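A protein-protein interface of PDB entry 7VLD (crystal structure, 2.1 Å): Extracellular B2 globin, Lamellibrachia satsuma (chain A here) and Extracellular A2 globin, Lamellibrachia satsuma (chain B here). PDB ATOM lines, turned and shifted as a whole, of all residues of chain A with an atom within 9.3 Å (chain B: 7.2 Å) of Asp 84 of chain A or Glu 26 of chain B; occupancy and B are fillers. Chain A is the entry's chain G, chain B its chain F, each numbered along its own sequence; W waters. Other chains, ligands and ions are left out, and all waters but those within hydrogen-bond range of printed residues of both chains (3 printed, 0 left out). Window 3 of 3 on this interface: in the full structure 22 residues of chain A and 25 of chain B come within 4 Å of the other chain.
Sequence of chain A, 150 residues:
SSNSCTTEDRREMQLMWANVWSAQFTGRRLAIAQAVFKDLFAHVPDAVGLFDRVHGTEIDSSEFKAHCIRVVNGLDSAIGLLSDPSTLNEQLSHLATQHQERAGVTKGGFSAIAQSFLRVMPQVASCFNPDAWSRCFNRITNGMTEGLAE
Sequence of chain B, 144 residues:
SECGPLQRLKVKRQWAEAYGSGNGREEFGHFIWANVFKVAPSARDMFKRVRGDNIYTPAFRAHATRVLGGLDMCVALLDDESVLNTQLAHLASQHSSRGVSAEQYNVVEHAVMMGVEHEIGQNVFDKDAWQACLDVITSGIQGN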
ATOM      1  N   ARG A  10      15.388  -7.170  26.986  1.00  0.00           N
ATOM      2  CA  ARG A  10      14.619  -8.408  27.085  1.00  0.00           C
ATOM      3  C   ARG A  10      14.187  -8.670  28.521  1.00  0.00           C
ATOM      4  O   ARG A  10      13.028  -9.019  28.777  1.00  0.00           O
ATOM      5  CB  ARG A  10      15.438  -9.581  26.545  1.00  0.00           C
ATOM      6  CG  ARG A  10      15.518  -9.618  25.031  1.00  0.00           C
ATOM      7  CD  ARG A  10      16.832 -10.200  24.534  1.00  0.00           C
ATOM      8  NE  ARG A  10      17.146  -9.713  23.193  1.00  0.00           N
ATOM      9  CZ  ARG A  10      16.964 -10.410  22.076  1.00  0.00           C
ATOM     10  NH1 ARG A  10      16.479 -11.643  22.129  1.00  0.00           N
ATOM     11  NH2 ARG A  10      17.276  -9.874  20.904  1.00  0.00           N
ATOM     12  N   GLN A  14      10.207  -8.850  29.758  1.00  0.00           N
ATOM     13  CA  GLN A  14       9.672  -9.981  30.504  1.00  0.00           C
ATOM     14  C   GLN A  14       9.155  -9.552  31.870  1.00  0.00           C
ATOM     15  O   GLN A  14       8.183 -10.126  32.370  1.00  0.00           O
ATOM     16  CB  GLN A  14      10.740 -11.066  30.643  1.00  0.00           C
ATOM     17  CG  GLN A  14      11.082 -11.749  29.327  1.00  0.00           C
ATOM     18  CD  GLN A  14      12.346 -12.581  29.403  1.00  0.00           C
ATOM     19  OE1 GLN A  14      13.176 -12.392  30.291  1.00  0.00           O
ATOM     20  NE2 GLN A  14      12.499 -13.509  28.464  1.00  0.00           N
ATOM     21  N   SER A  77       4.593 -16.535  24.334  1.00  0.00           N
ATOM     22  CA  SER A  77       5.607 -17.488  23.893  1.00  0.00           C
ATOM     23  C   SER A  77       6.814 -16.769  23.308  1.00  0.00           C
ATOM     24  O   SER A  77       7.958 -17.190  23.511  1.00  0.00           O
ATOM     25  CB  SER A  77       5.014 -18.458  22.871  1.00  0.00           C
ATOM     26  OG  SER A  77       4.830 -17.829  21.612  1.00  0.00           O
ATOM     27  N   ALA A  78       6.579 -15.672  22.584  1.00  0.00           N
ATOM     28  CA  ALA A  78       7.685 -14.916  22.006  1.00  0.00           C
ATOM     29  C   ALA A  78       8.472 -14.184  23.086  1.00  0.00           C
ATOM     30  O   ALA A  78       9.709 -14.227  23.103  1.00  0.00           O
ATOM     31  CB  ALA A  78       7.157 -13.936  20.960  1.00  0.00           C
ATOM     32  N   ILE A  79       7.770 -13.509  24.001  1.00  0.00           N
ATOM     33  CA  ILE A  79       8.440 -12.755  25.059  1.00  0.00           C
ATOM     34  C   ILE A  79       9.301 -13.678  25.913  1.00  0.00           C
ATOM     35  O   ILE A  79      10.431 -13.335  26.281  1.00  0.00           O
ATOM     36  CB  ILE A  79       7.403 -11.993  25.907  1.00  0.00           C
ATOM     37  CG1 ILE A  79       6.774 -10.861  25.087  1.00  0.00           C
ATOM     38  CG2 ILE A  79       8.038 -11.449  27.178  1.00  0.00           C
ATOM     39  CD1 ILE A  79       5.738 -10.056  25.843  1.00  0.00           C
ATOM     40  N   GLY A  80       8.788 -14.868  26.231  1.00  0.00           N
ATOM     41  CA  GLY A  80       9.566 -15.815  27.010  1.00  0.00           C
ATOM     42  C   GLY A  80      10.756 -16.378  26.258  1.00  0.00           C
ATOM     43  O   GLY A  80      11.798 -16.654  26.859  1.00  0.00           O
ATOM     44  N   LEU A  81      10.626 -16.553  24.944  1.00  0.00           N
ATOM     45  CA  LEU A  81      11.715 -17.086  24.136  1.00  0.00           C
ATOM     46  C   LEU A  81      12.750 -16.035  23.759  1.00  0.00           C
ATOM     47  O   LEU A  81      13.731 -16.376  23.090  1.00  0.00           O
ATOM     48  CB  LEU A  81      11.159 -17.749  22.874  1.00  0.00           C
ATOM     49  CG  LEU A  81      10.523 -19.120  23.114  1.00  0.00           C
ATOM     50  CD1 LEU A  81       9.932 -19.682  21.831  1.00  0.00           C
ATOM     51  CD2 LEU A  81      11.548 -20.076  23.704  1.00  0.00           C
ATOM     52  N   LEU A  82      12.564 -14.777  24.167  1.00  0.00           N
ATOM     53  CA  LEU A  82      13.618 -13.781  24.009  1.00  0.00           C
ATOM     54  C   LEU A  82      14.903 -14.193  24.714  1.00  0.00           C
ATOM     55  O   LEU A  82      15.978 -13.695  24.364  1.00  0.00           O
ATOM     56  CB  LEU A  82      13.154 -12.421  24.541  1.00  0.00           C
ATOM     57  CG  LEU A  82      12.113 -11.640  23.738  1.00  0.00           C
ATOM     58  CD1 LEU A  82      11.654 -10.416  24.518  1.00  0.00           C
ATOM     59  CD2 LEU A  82      12.668 -11.233  22.381  1.00  0.00           C
ATOM     60  N   SER A  83      14.814 -15.088  25.700  1.00  0.00           N
ATOM     61  CA  SER A  83      15.982 -15.592  26.409  1.00  0.00           C
ATOM     62  C   SER A  83      16.676 -16.734  25.677  1.00  0.00           C
ATOM     63  O   SER A  83      17.770 -17.133  26.088  1.00  0.00           O
ATOM     64  CB  SER A  83      15.582 -16.058  27.811  1.00  0.00           C
ATOM     65  OG  SER A  83      14.889 -15.040  28.512  1.00  0.00           O
ATOM     66  N   ASP A  84      16.068 -17.271  24.624  1.00  0.00           N
ATOM     67  CA  ASP A  84      16.661 -18.341  23.821  1.00  0.00           C
ATOM     68  C   ASP A  84      16.388 -18.032  22.358  1.00  0.00           C
ATOM     69  O   ASP A  84      15.470 -18.592  21.746  1.00  0.00           O
ATOM     70  CB  ASP A  84      16.098 -19.708  24.217  1.00  0.00           C
ATOM     71  CG  ASP A  84      16.746 -20.850  23.458  1.00  0.00           C
ATOM     72  OD1 ASP A  84      17.847 -20.649  22.901  1.00  0.00           O
ATOM     73  OD2 ASP A  84      16.152 -21.947  23.414  1.00  0.00           O
ATOM     74  N   PRO A  85      17.171 -17.129  21.761  1.00  0.00           N
ATOM     75  CA  PRO A  85      16.843 -16.660  20.404  1.00  0.00           C
ATOM     76  C   PRO A  85      16.889 -17.745  19.343  1.00  0.00           C
ATOM     77  O   PRO A  85      16.208 -17.614  18.317  1.00  0.00           O
ATOM     78  CB  PRO A  85      17.897 -15.572  20.151  1.00  0.00           C
ATOM     79  CG  PRO A  85      18.305 -15.123  21.519  1.00  0.00           C
ATOM     80  CD  PRO A  85      18.280 -16.366  22.355  1.00  0.00           C
ATOM     81  N   SER A  86      17.675 -18.805  19.547  1.00  0.00           N
ATOM     82  CA  SER A  86      17.659 -19.927  18.612  1.00  0.00           C
ATOM     83  C   SER A  86      16.254 -20.502  18.481  1.00  0.00           C
ATOM     84  O   SER A  86      15.735 -20.663  17.371  1.00  0.00           O
ATOM     85  CB  SER A  86      18.641 -21.006  19.069  1.00  0.00           C
ATOM     86  OG  SER A  86      19.954 -20.489  19.184  1.00  0.00           O
ATOM     87  N   THR A  87      15.620 -20.808  19.614  1.00  0.00           N
ATOM     88  CA  THR A  87      14.254 -21.317  19.584  1.00  0.00           C
ATOM     89  C   THR A  87      13.264 -20.233  19.175  1.00  0.00           C
ATOM     90  O   THR A  87      12.263 -20.529  18.512  1.00  0.00           O
ATOM     91  CB  THR A  87      13.889 -21.898  20.951  1.00  0.00           C
ATOM     92  OG1 THR A  87      14.861 -22.885  21.322  1.00  0.00           O
ATOM     93  CG2 THR A  87      12.513 -22.544  20.916  1.00  0.00           C
ATOM     94  N   LEU A  88      13.533 -18.978  19.548  1.00  0.00           N
ATOM     95  CA  LEU A  88      12.646 -17.880  19.172  1.00  0.00           C
ATOM     96  C   LEU A  88      12.491 -17.780  17.660  1.00  0.00           C
ATOM     97  O   LEU A  88      11.376 -17.599  17.155  1.00  0.00           O
ATOM     98  CB  LEU A  88      13.173 -16.562  19.738  1.00  0.00           C
ATOM     99  CG  LEU A  88      12.418 -15.300  19.315  1.00  0.00           C
ATOM    100  CD1 LEU A  88      11.015 -15.281  19.907  1.00  0.00           C
ATOM    101  CD2 LEU A  88      13.192 -14.048  19.705  1.00  0.00           C
ATOM    102  N   ASN A  89      13.597 -17.898  16.920  1.00  0.00           N
ATOM    103  CA  ASN A  89      13.530 -17.780  15.466  1.00  0.00           C
ATOM    104  C   ASN A  89      12.640 -18.860  14.862  1.00  0.00           C
ATOM    105  O   ASN A  89      11.919 -18.608  13.890  1.00  0.00           O
ATOM    106  CB  ASN A  89      14.936 -17.839  14.869  1.00  0.00           C
ATOM    107  CG  ASN A  89      15.737 -16.580  15.142  1.00  0.00           C
ATOM    108  OD1 ASN A  89      15.179 -15.490  15.267  1.00  0.00           O
ATOM    109  ND2 ASN A  89      17.055 -16.722  15.234  1.00  0.00           N
ATOM    110  N   GLU A  90      12.673 -20.068  15.430  1.00  0.00           N
ATOM    111  CA  GLU A  90      11.788 -21.129  14.960  1.00  0.00           C
ATOM    112  C   GLU A  90      10.327 -20.797  15.244  1.00  0.00           C
ATOM    113  O   GLU A  90       9.460 -21.003  14.387  1.00  0.00           O
ATOM    114  CB  GLU A  90      12.171 -22.458  15.609  1.00  0.00           C
ATOM    115  CG  GLU A  90      13.583 -22.918  15.291  1.00  0.00           C
ATOM    116  CD  GLU A  90      13.790 -23.165  13.812  1.00  0.00           C
ATOM    117  OE1 GLU A  90      12.916 -23.801  13.187  1.00  0.00           O
ATOM    118  OE2 GLU A  90      14.822 -22.715  13.272  1.00  0.00           O
ATOM    119  N   GLN A  91      10.038 -20.276  16.440  1.00  0.00           N
ATOM    120  CA  GLN A  91       8.657 -19.972  16.804  1.00  0.00           C
ATOM    121  C   GLN A  91       8.108 -18.811  15.987  1.00  0.00           C
ATOM    122  O   GLN A  91       6.932 -18.816  15.603  1.00  0.00           O
ATOM    123  CB  GLN A  91       8.566 -19.669  18.300  1.00  0.00           C
ATOM    124  CG  GLN A  91       7.192 -19.207  18.778  1.00  0.00           C
ATOM    125  CD  GLN A  91       6.157 -20.319  18.795  1.00  0.00           C
ATOM    126  OE1 GLN A  91       6.430 -21.448  18.384  1.00  0.00           O
ATOM    127  NE2 GLN A  91       4.962 -20.005  19.277  1.00  0.00           N
ATOM    128  N   LEU A  92       8.941 -17.804  15.712  1.00  0.00           N
ATOM    129  CA  LEU A  92       8.489 -16.678  14.904  1.00  0.00           C
ATOM    130  C   LEU A  92       8.257 -17.085  13.453  1.00  0.00           C
ATOM    131  O   LEU A  92       7.377 -16.526  12.789  1.00  0.00           O
ATOM    132  CB  LEU A  92       9.497 -15.532  14.984  1.00  0.00           C
ATOM    133  CG  LEU A  92       9.702 -14.917  16.372  1.00  0.00           C
ATOM    134  CD1 LEU A  92      10.602 -13.694  16.292  1.00  0.00           C
ATOM    135  CD2 LEU A  92       8.368 -14.570  17.020  1.00  0.00           C
ATOM    136  N   ARG A 139      11.370  -6.412  17.392  1.00  0.00           N
ATOM    137  CA  ARG A 139      12.168  -7.609  17.143  1.00  0.00           C
ATOM    138  C   ARG A 139      11.283  -8.832  16.946  1.00  0.00           C
ATOM    139  O   ARG A 139      11.601  -9.710  16.136  1.00  0.00           O
ATOM    140  CB  ARG A 139      13.143  -7.833  18.304  1.00  0.00           C
ATOM    141  CG  ARG A 139      13.702  -9.248  18.415  1.00  0.00           C
ATOM    142  CD  ARG A 139      14.706  -9.551  17.315  1.00  0.00           C
ATOM    143  NE  ARG A 139      15.229 -10.911  17.413  1.00  0.00           N
ATOM    144  CZ  ARG A 139      14.724 -11.955  16.763  1.00  0.00           C
ATOM    145  NH1 ARG A 139      13.679 -11.796  15.962  1.00  0.00           N
ATOM    146  NH2 ARG A 139      15.264 -13.157  16.911  1.00  0.00           N
ATOM    147  N   TYR B  19       4.341 -24.649  35.399  1.00  0.00           N
ATOM    148  CA  TYR B  19       4.614 -23.919  34.165  1.00  0.00           C
ATOM    149  C   TYR B  19       5.458 -22.680  34.434  1.00  0.00           C
ATOM    150  O   TYR B  19       6.340 -22.337  33.637  1.00  0.00           O
ATOM    151  CB  TYR B  19       3.290 -23.550  33.495  1.00  0.00           C
ATOM    152  CG  TYR B  19       3.385 -23.080  32.061  1.00  0.00           C
ATOM    153  CD1 TYR B  19       4.199 -23.729  31.142  1.00  0.00           C
ATOM    154  CD2 TYR B  19       2.625 -22.007  31.620  1.00  0.00           C
ATOM    155  CE1 TYR B  19       4.270 -23.302  29.825  1.00  0.00           C
ATOM    156  CE2 TYR B  19       2.687 -21.575  30.312  1.00  0.00           C
ATOM    157  CZ  TYR B  19       3.509 -22.224  29.418  1.00  0.00           C
ATOM    158  OH  TYR B  19       3.566 -21.786  28.114  1.00  0.00           O
ATOM    159  N   GLY B  22       8.501 -18.524  32.924  1.00  0.00           N
ATOM    160  CA  GLY B  22       9.220 -18.713  31.680  1.00  0.00           C
ATOM    161  C   GLY B  22      10.628 -19.255  31.820  1.00  0.00           C
ATOM    162  O   GLY B  22      11.130 -19.924  30.910  1.00  0.00           O
ATOM    163  N   ASN B  23      11.273 -18.981  32.957  1.00  0.00           N
ATOM    164  CA  ASN B  23      12.682 -19.333  33.116  1.00  0.00           C
ATOM    165  C   ASN B  23      12.907 -20.839  33.066  1.00  0.00           C
ATOM    166  O   ASN B  23      13.946 -21.294  32.573  1.00  0.00           O
ATOM    167  CB  ASN B  23      13.217 -18.758  34.429  1.00  0.00           C
ATOM    168  CG  ASN B  23      13.046 -17.253  34.519  1.00  0.00           C
ATOM    169  OD1 ASN B  23      11.987 -16.760  34.908  1.00  0.00           O
ATOM    170  ND2 ASN B  23      14.090 -16.516  34.159  1.00  0.00           N
ATOM    171  N   GLY B  24      11.954 -21.628  33.563  1.00  0.00           N
ATOM    172  CA  GLY B  24      12.077 -23.072  33.568  1.00  0.00           C
ATOM    173  C   GLY B  24      11.204 -23.817  32.584  1.00  0.00           C
ATOM    174  O   GLY B  24      11.067 -25.040  32.707  1.00  0.00           O
ATOM    175  N   ARG B  25      10.609 -23.133  31.604  1.00  0.00           N
ATOM    176  CA  ARG B  25       9.701 -23.807  30.681  1.00  0.00           C
ATOM    177  C   ARG B  25      10.441 -24.747  29.737  1.00  0.00           C
ATOM    178  O   ARG B  25       9.879 -25.766  29.318  1.00  0.00           O
ATOM    179  CB  ARG B  25       8.897 -22.776  29.887  1.00  0.00           C
ATOM    180  CG  ARG B  25       7.868 -22.028  30.720  1.00  0.00           C
ATOM    181  CD  ARG B  25       7.102 -21.012  29.888  1.00  0.00           C
ATOM    182  NE  ARG B  25       6.124 -20.283  30.691  1.00  0.00           N
ATOM    183  CZ  ARG B  25       5.405 -19.256  30.247  1.00  0.00           C
ATOM    184  NH1 ARG B  25       5.552 -18.828  29.000  1.00  0.00           N
ATOM    185  NH2 ARG B  25       4.538 -18.654  31.051  1.00  0.00           N
ATOM    186  N   GLU B  26      11.692 -24.428  29.394  1.00  0.00           N
ATOM    187  CA  GLU B  26      12.463 -25.298  28.510  1.00  0.00           C
ATOM    188  C   GLU B  26      12.671 -26.671  29.137  1.00  0.00           C
ATOM    189  O   GLU B  26      12.382 -27.700  28.515  1.00  0.00           O
ATOM    190  CB  GLU B  26      13.808 -24.651  28.177  1.00  0.00           C
ATOM    191  CG  GLU B  26      14.633 -25.429  27.160  1.00  0.00           C
ATOM    192  CD  GLU B  26      16.062 -24.929  27.054  1.00  0.00           C
ATOM    193  OE1 GLU B  26      16.875 -25.259  27.943  1.00  0.00           O
ATOM    194  OE2 GLU B  26      16.370 -24.202  26.086  1.00  0.00           O
ATOM    195  N   GLU B  27      13.174 -26.703  30.373  1.00  0.00           N
ATOM    196  CA  GLU B  27      13.364 -27.972  31.070  1.00  0.00           C
ATOM    197  C   GLU B  27      12.035 -28.687  31.280  1.00  0.00           C
ATOM    198  O   GLU B  27      11.960 -29.917  31.173  1.00  0.00           O
ATOM    199  CB  GLU B  27      14.067 -27.729  32.409  1.00  0.00           C
ATOM    200  CG  GLU B  27      14.388 -28.985  33.220  1.00  0.00           C
ATOM    201  CD  GLU B  27      13.223 -29.467  34.071  1.00  0.00           C
ATOM    202  OE1 GLU B  27      13.127 -30.688  34.312  1.00  0.00           O
ATOM    203  OE2 GLU B  27      12.402 -28.625  34.494  1.00  0.00           O
ATOM    204  N   PHE B  28      10.978 -27.930  31.583  1.00  0.00           N
ATOM    205  CA  PHE B  28       9.664 -28.524  31.808  1.00  0.00           C
ATOM    206  C   PHE B  28       9.162 -29.234  30.556  1.00  0.00           C
ATOM    207  O   PHE B  28       8.755 -30.401  30.610  1.00  0.00           O
ATOM    208  CB  PHE B  28       8.683 -27.436  32.254  1.00  0.00           C
ATOM    209  CG  PHE B  28       7.305 -27.943  32.589  1.00  0.00           C
ATOM    210  CD1 PHE B  28       7.131 -29.084  33.353  1.00  0.00           C
ATOM    211  CD2 PHE B  28       6.182 -27.253  32.161  1.00  0.00           C
ATOM    212  CE1 PHE B  28       5.861 -29.539  33.667  1.00  0.00           C
ATOM    213  CE2 PHE B  28       4.912 -27.701  32.472  1.00  0.00           C
ATOM    214  CZ  PHE B  28       4.752 -28.846  33.225  1.00  0.00           C
ATOM    215  N   GLY B  29       9.194 -28.545  29.414  1.00  0.00           N
ATOM    216  CA  GLY B  29       8.767 -29.173  28.174  1.00  0.00           C
ATOM    217  C   GLY B  29       9.642 -30.348  27.782  1.00  0.00           C
ATOM    218  O   GLY B  29       9.149 -31.359  27.278  1.00  0.00           O
ATOM    219  N   HIS B  30      10.952 -30.234  28.016  1.00  0.00           N
ATOM    220  CA  HIS B  30      11.862 -31.319  27.667  1.00  0.00           C
ATOM    221  C   HIS B  30      11.570 -32.572  28.482  1.00  0.00           C
ATOM    222  O   HIS B  30      11.573 -33.685  27.943  1.00  0.00           O
ATOM    223  CB  HIS B  30      13.310 -30.881  27.867  1.00  0.00           C
ATOM    224  CG  HIS B  30      14.306 -31.959  27.577  1.00  0.00           C
ATOM    225  ND1 HIS B  30      14.866 -32.741  28.564  1.00  0.00           N
ATOM    226  CD2 HIS B  30      14.831 -32.395  26.407  1.00  0.00           C
ATOM    227  CE1 HIS B  30      15.699 -33.608  28.016  1.00  0.00           C
ATOM    228  NE2 HIS B  30      15.695 -33.420  26.709  1.00  0.00           N
ATOM    229  N   PHE B  31      11.324 -32.411  29.785  1.00  0.00           N
ATOM    230  CA  PHE B  31      10.996 -33.557  30.629  1.00  0.00           C
ATOM    231  C   PHE B  31       9.742 -34.263  30.130  1.00  0.00           C
ATOM    232  O   PHE B  31       9.686 -35.499  30.101  1.00  0.00           O
ATOM    233  CB  PHE B  31      10.816 -33.101  32.079  1.00  0.00           C
ATOM    234  CG  PHE B  31      10.637 -34.230  33.061  1.00  0.00           C
ATOM    235  CD1 PHE B  31       9.390 -34.797  33.273  1.00  0.00           C
ATOM    236  CD2 PHE B  31      11.717 -34.710  33.785  1.00  0.00           C
ATOM    237  CE1 PHE B  31       9.226 -35.830  34.178  1.00  0.00           C
ATOM    238  CE2 PHE B  31      11.558 -35.741  34.693  1.00  0.00           C
ATOM    239  CZ  PHE B  31      10.311 -36.302  34.889  1.00  0.00           C
ATOM    240  N   ILE B  32       8.728 -33.494  29.728  1.00  0.00           N
ATOM    241  CA  ILE B  32       7.471 -34.086  29.277  1.00  0.00           C
ATOM    242  C   ILE B  32       7.687 -34.889  27.999  1.00  0.00           C
ATOM    243  O   ILE B  32       7.274 -36.050  27.896  1.00  0.00           O
ATOM    244  CB  ILE B  32       6.405 -32.993  29.085  1.00  0.00           C
ATOM    245  CG1 ILE B  32       6.010 -32.390  30.436  1.00  0.00           C
ATOM    246  CG2 ILE B  32       5.190 -33.548  28.352  1.00  0.00           C
ATOM    247  CD1 ILE B  32       5.178 -31.134  30.327  1.00  0.00           C
ATOM    248  N   TYR B  56      16.285 -31.930  21.269  1.00  0.00           N
ATOM    249  CA  TYR B  56      17.228 -30.909  21.706  1.00  0.00           C
ATOM    250  C   TYR B  56      17.369 -29.762  20.713  1.00  0.00           C
ATOM    251  O   TYR B  56      18.035 -28.769  21.027  1.00  0.00           O
ATOM    252  CB  TYR B  56      18.607 -31.531  21.953  1.00  0.00           C
ATOM    253  CG  TYR B  56      18.597 -32.684  22.929  1.00  0.00           C
ATOM    254  CD1 TYR B  56      18.411 -33.988  22.488  1.00  0.00           C
ATOM    255  CD2 TYR B  56      18.776 -32.472  24.290  1.00  0.00           C
ATOM    256  CE1 TYR B  56      18.402 -35.047  23.376  1.00  0.00           C
ATOM    257  CE2 TYR B  56      18.769 -33.525  25.185  1.00  0.00           C
ATOM    258  CZ  TYR B  56      18.582 -34.810  24.722  1.00  0.00           C
ATOM    259  OH  TYR B  56      18.574 -35.863  25.609  1.00  0.00           O
ATOM    260  N   PRO B  58      16.320 -26.459  18.403  1.00  0.00           N
ATOM    261  CA  PRO B  58      15.385 -25.330  18.537  1.00  0.00           C
ATOM    262  C   PRO B  58      14.063 -25.563  17.830  1.00  0.00           C
ATOM    263  O   PRO B  58      13.033 -25.031  18.267  1.00  0.00           O
ATOM    264  CB  PRO B  58      16.162 -24.161  17.915  1.00  0.00           C
ATOM    265  CG  PRO B  58      17.596 -24.540  18.078  1.00  0.00           C
ATOM    266  CD  PRO B  58      17.639 -26.031  17.907  1.00  0.00           C
ATOM    267  N   ARG B  61      12.052 -27.656  20.307  1.00  0.00           N
ATOM    268  CA  ARG B  61      11.777 -26.831  21.477  1.00  0.00           C
ATOM    269  C   ARG B  61      10.708 -25.791  21.177  1.00  0.00           C
ATOM    270  O   ARG B  61       9.941 -25.411  22.069  1.00  0.00           O
ATOM    271  CB  ARG B  61      13.062 -26.159  21.964  1.00  0.00           C
ATOM    272  CG  ARG B  61      14.144 -27.133  22.417  1.00  0.00           C
ATOM    273  CD  ARG B  61      15.332 -26.399  23.025  1.00  0.00           C
ATOM    274  NE  ARG B  61      16.483 -27.273  23.241  1.00  0.00           N
ATOM    275  CZ  ARG B  61      16.652 -28.044  24.310  1.00  0.00           C
ATOM    276  NH1 ARG B  61      17.736 -28.801  24.418  1.00  0.00           N
ATOM    277  NH2 ARG B  61      15.737 -28.066  25.270  1.00  0.00           N
ATOM    278  N   ALA B  64       7.448 -27.837  21.363  1.00  0.00           N
ATOM    279  CA  ALA B  64       7.099 -28.042  22.765  1.00  0.00           C
ATOM    280  C   ALA B  64       6.555 -26.767  23.392  1.00  0.00           C
ATOM    281  O   ALA B  64       5.664 -26.827  24.247  1.00  0.00           O
ATOM    282  CB  ALA B  64       8.312 -28.544  23.546  1.00  0.00           C
ATOM    283  N   THR B  65       7.073 -25.608  22.979  1.00  0.00           N
ATOM    284  CA  THR B  65       6.531 -24.342  23.457  1.00  0.00           C
ATOM    285  C   THR B  65       5.076 -24.178  23.036  1.00  0.00           C
ATOM    286  O   THR B  65       4.237 -23.733  23.829  1.00  0.00           O
ATOM    287  CB  THR B  65       7.379 -23.181  22.934  1.00  0.00           C
ATOM    288  OG1 THR B  65       8.705 -23.273  23.473  1.00  0.00           O
ATOM    289  CG2 THR B  65       6.768 -21.843  23.328  1.00  0.00           C
ATOM    290  N   LEU B  68       2.795 -26.744  25.163  1.00  0.00           N
ATOM    291  CA  LEU B  68       2.562 -26.274  26.524  1.00  0.00           C
ATOM    292  C   LEU B  68       1.743 -24.990  26.539  1.00  0.00           C
ATOM    293  O   LEU B  68       0.957 -24.767  27.467  1.00  0.00           O
ATOM    294  CB  LEU B  68       3.890 -26.063  27.253  1.00  0.00           C
ATOM    295  CG  LEU B  68       4.835 -27.263  27.386  1.00  0.00           C
ATOM    296  CD1 LEU B  68       5.834 -27.037  28.513  1.00  0.00           C
ATOM    297  CD2 LEU B  68       4.067 -28.559  27.594  1.00  0.00           C
HETATM  298  O   HOH W   1      14.349 -22.715  25.109  1.00  0.00           O
HETATM  299  O   HOH W   2       6.745 -15.726  28.836  1.00  0.00           O
HETATM  300  O   HOH W   3       3.448 -19.344  25.620  1.00  0.00           O
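Water W1 lies within hydrogen-bond range of the side-chain carboxylate (OD2) of Asp 84 of chain A and the side-chain carboxylate (OE2) of Glu 26 of chain B.
Water W3 lies within hydrogen-bond range of the backbone NH (N) of Ser 77 of chain A (3.3 Å) and the side-chain hydroxyl (OH) of Tyr 19 of chain B (3.5 Å).
Water W2 lies within hydrogen-bond range of the guanidinium group of Arg 25 of chain B (3.3 Å) and the backbone NH of Gly 80 of chain A (3.4 Å).
Among the printed residues, merely in contact across the chains: Asp 84 of chain A with Glu 26 of chain B, Ser 86 of chain A with Pro 58 of chain B, Thr 87 of chain A with Pro 58 of chain B, Glu 90 of chain A with Pro 58 of chain B, Thr 87 of chain A with Arg 61 of chain B and Ser 77 of chain A with Thr 65 of chain B.
The backbone carbonyl oxygen of Tyr 56 of chain B lies within hydrogen-bond range of the guanidinium group of Arg 61 of chain B (3.1 Å).
OG of Ser 77 of chain A is in hydrogen-bond range of NE2 of Gln 91 of chain A, at 3.2 Å.
The side-chain carboxylate of Asp 84 of chain A is in hydrogen-bond range of the side-chain hydroxyl of Thr 87 of chain A, at 2.6 Å.
O of Arg 61 of chain B sits at hydrogen-bond distance from OG1 of Thr 65 of chain B (2.8 Å).
The side-chain carboxylate (OE2) of Glu 26 of chain B is in salt-bridge range of the guanidinium group (NH2) of Arg 61 of chain B, at 3.9996 Å.
Asp 84 of chain A touches one residue of chain B.
Asn 89 of chain A touches none of the printed residues of chain B.
Of the printed residues of chain B, Glu 90 of chain A touches Pro 58 (3.7 Å).
No residue of chain A comes within 4 Å of Gly 24 of chain B.
Glu 26 of chain B touches just one residue of chain A: Asp 84.
No residue of chain A comes within 4 Å of Gly 29 of chain B.
Of the printed residues of chain A, Arg 61 of chain B touches Thr 87.
Printed residues of chain A within 4 Å of Thr 65 of chain B: Ser 77.
The nearest residue of chain A that does not touch Glu 26 of chain B is Thr 87 of chain A (5.2 Å).
The nearest printed residue of chain B that does not touch Glu 90 of chain A is Arg 61 of chain B (6.7 Å).
Of the 19 printed residues of chain A, 5 touch a printed residue of chain B.
Printed residues of chain A that touch a printed residue of chain B: Ser 77, Asp 84, Ser 86, Thr 87 and Glu 90.
Along chain A the printed residues that touch a printed residue of chain B span positions 77 to 90.
Printed residues of chain B that touch a printed residue of chain A: Glu 26, Pro 58, Arg 61 and Thr 65.
Along chain B the printed residues that touch a printed residue of chain A span positions 26 to 65.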
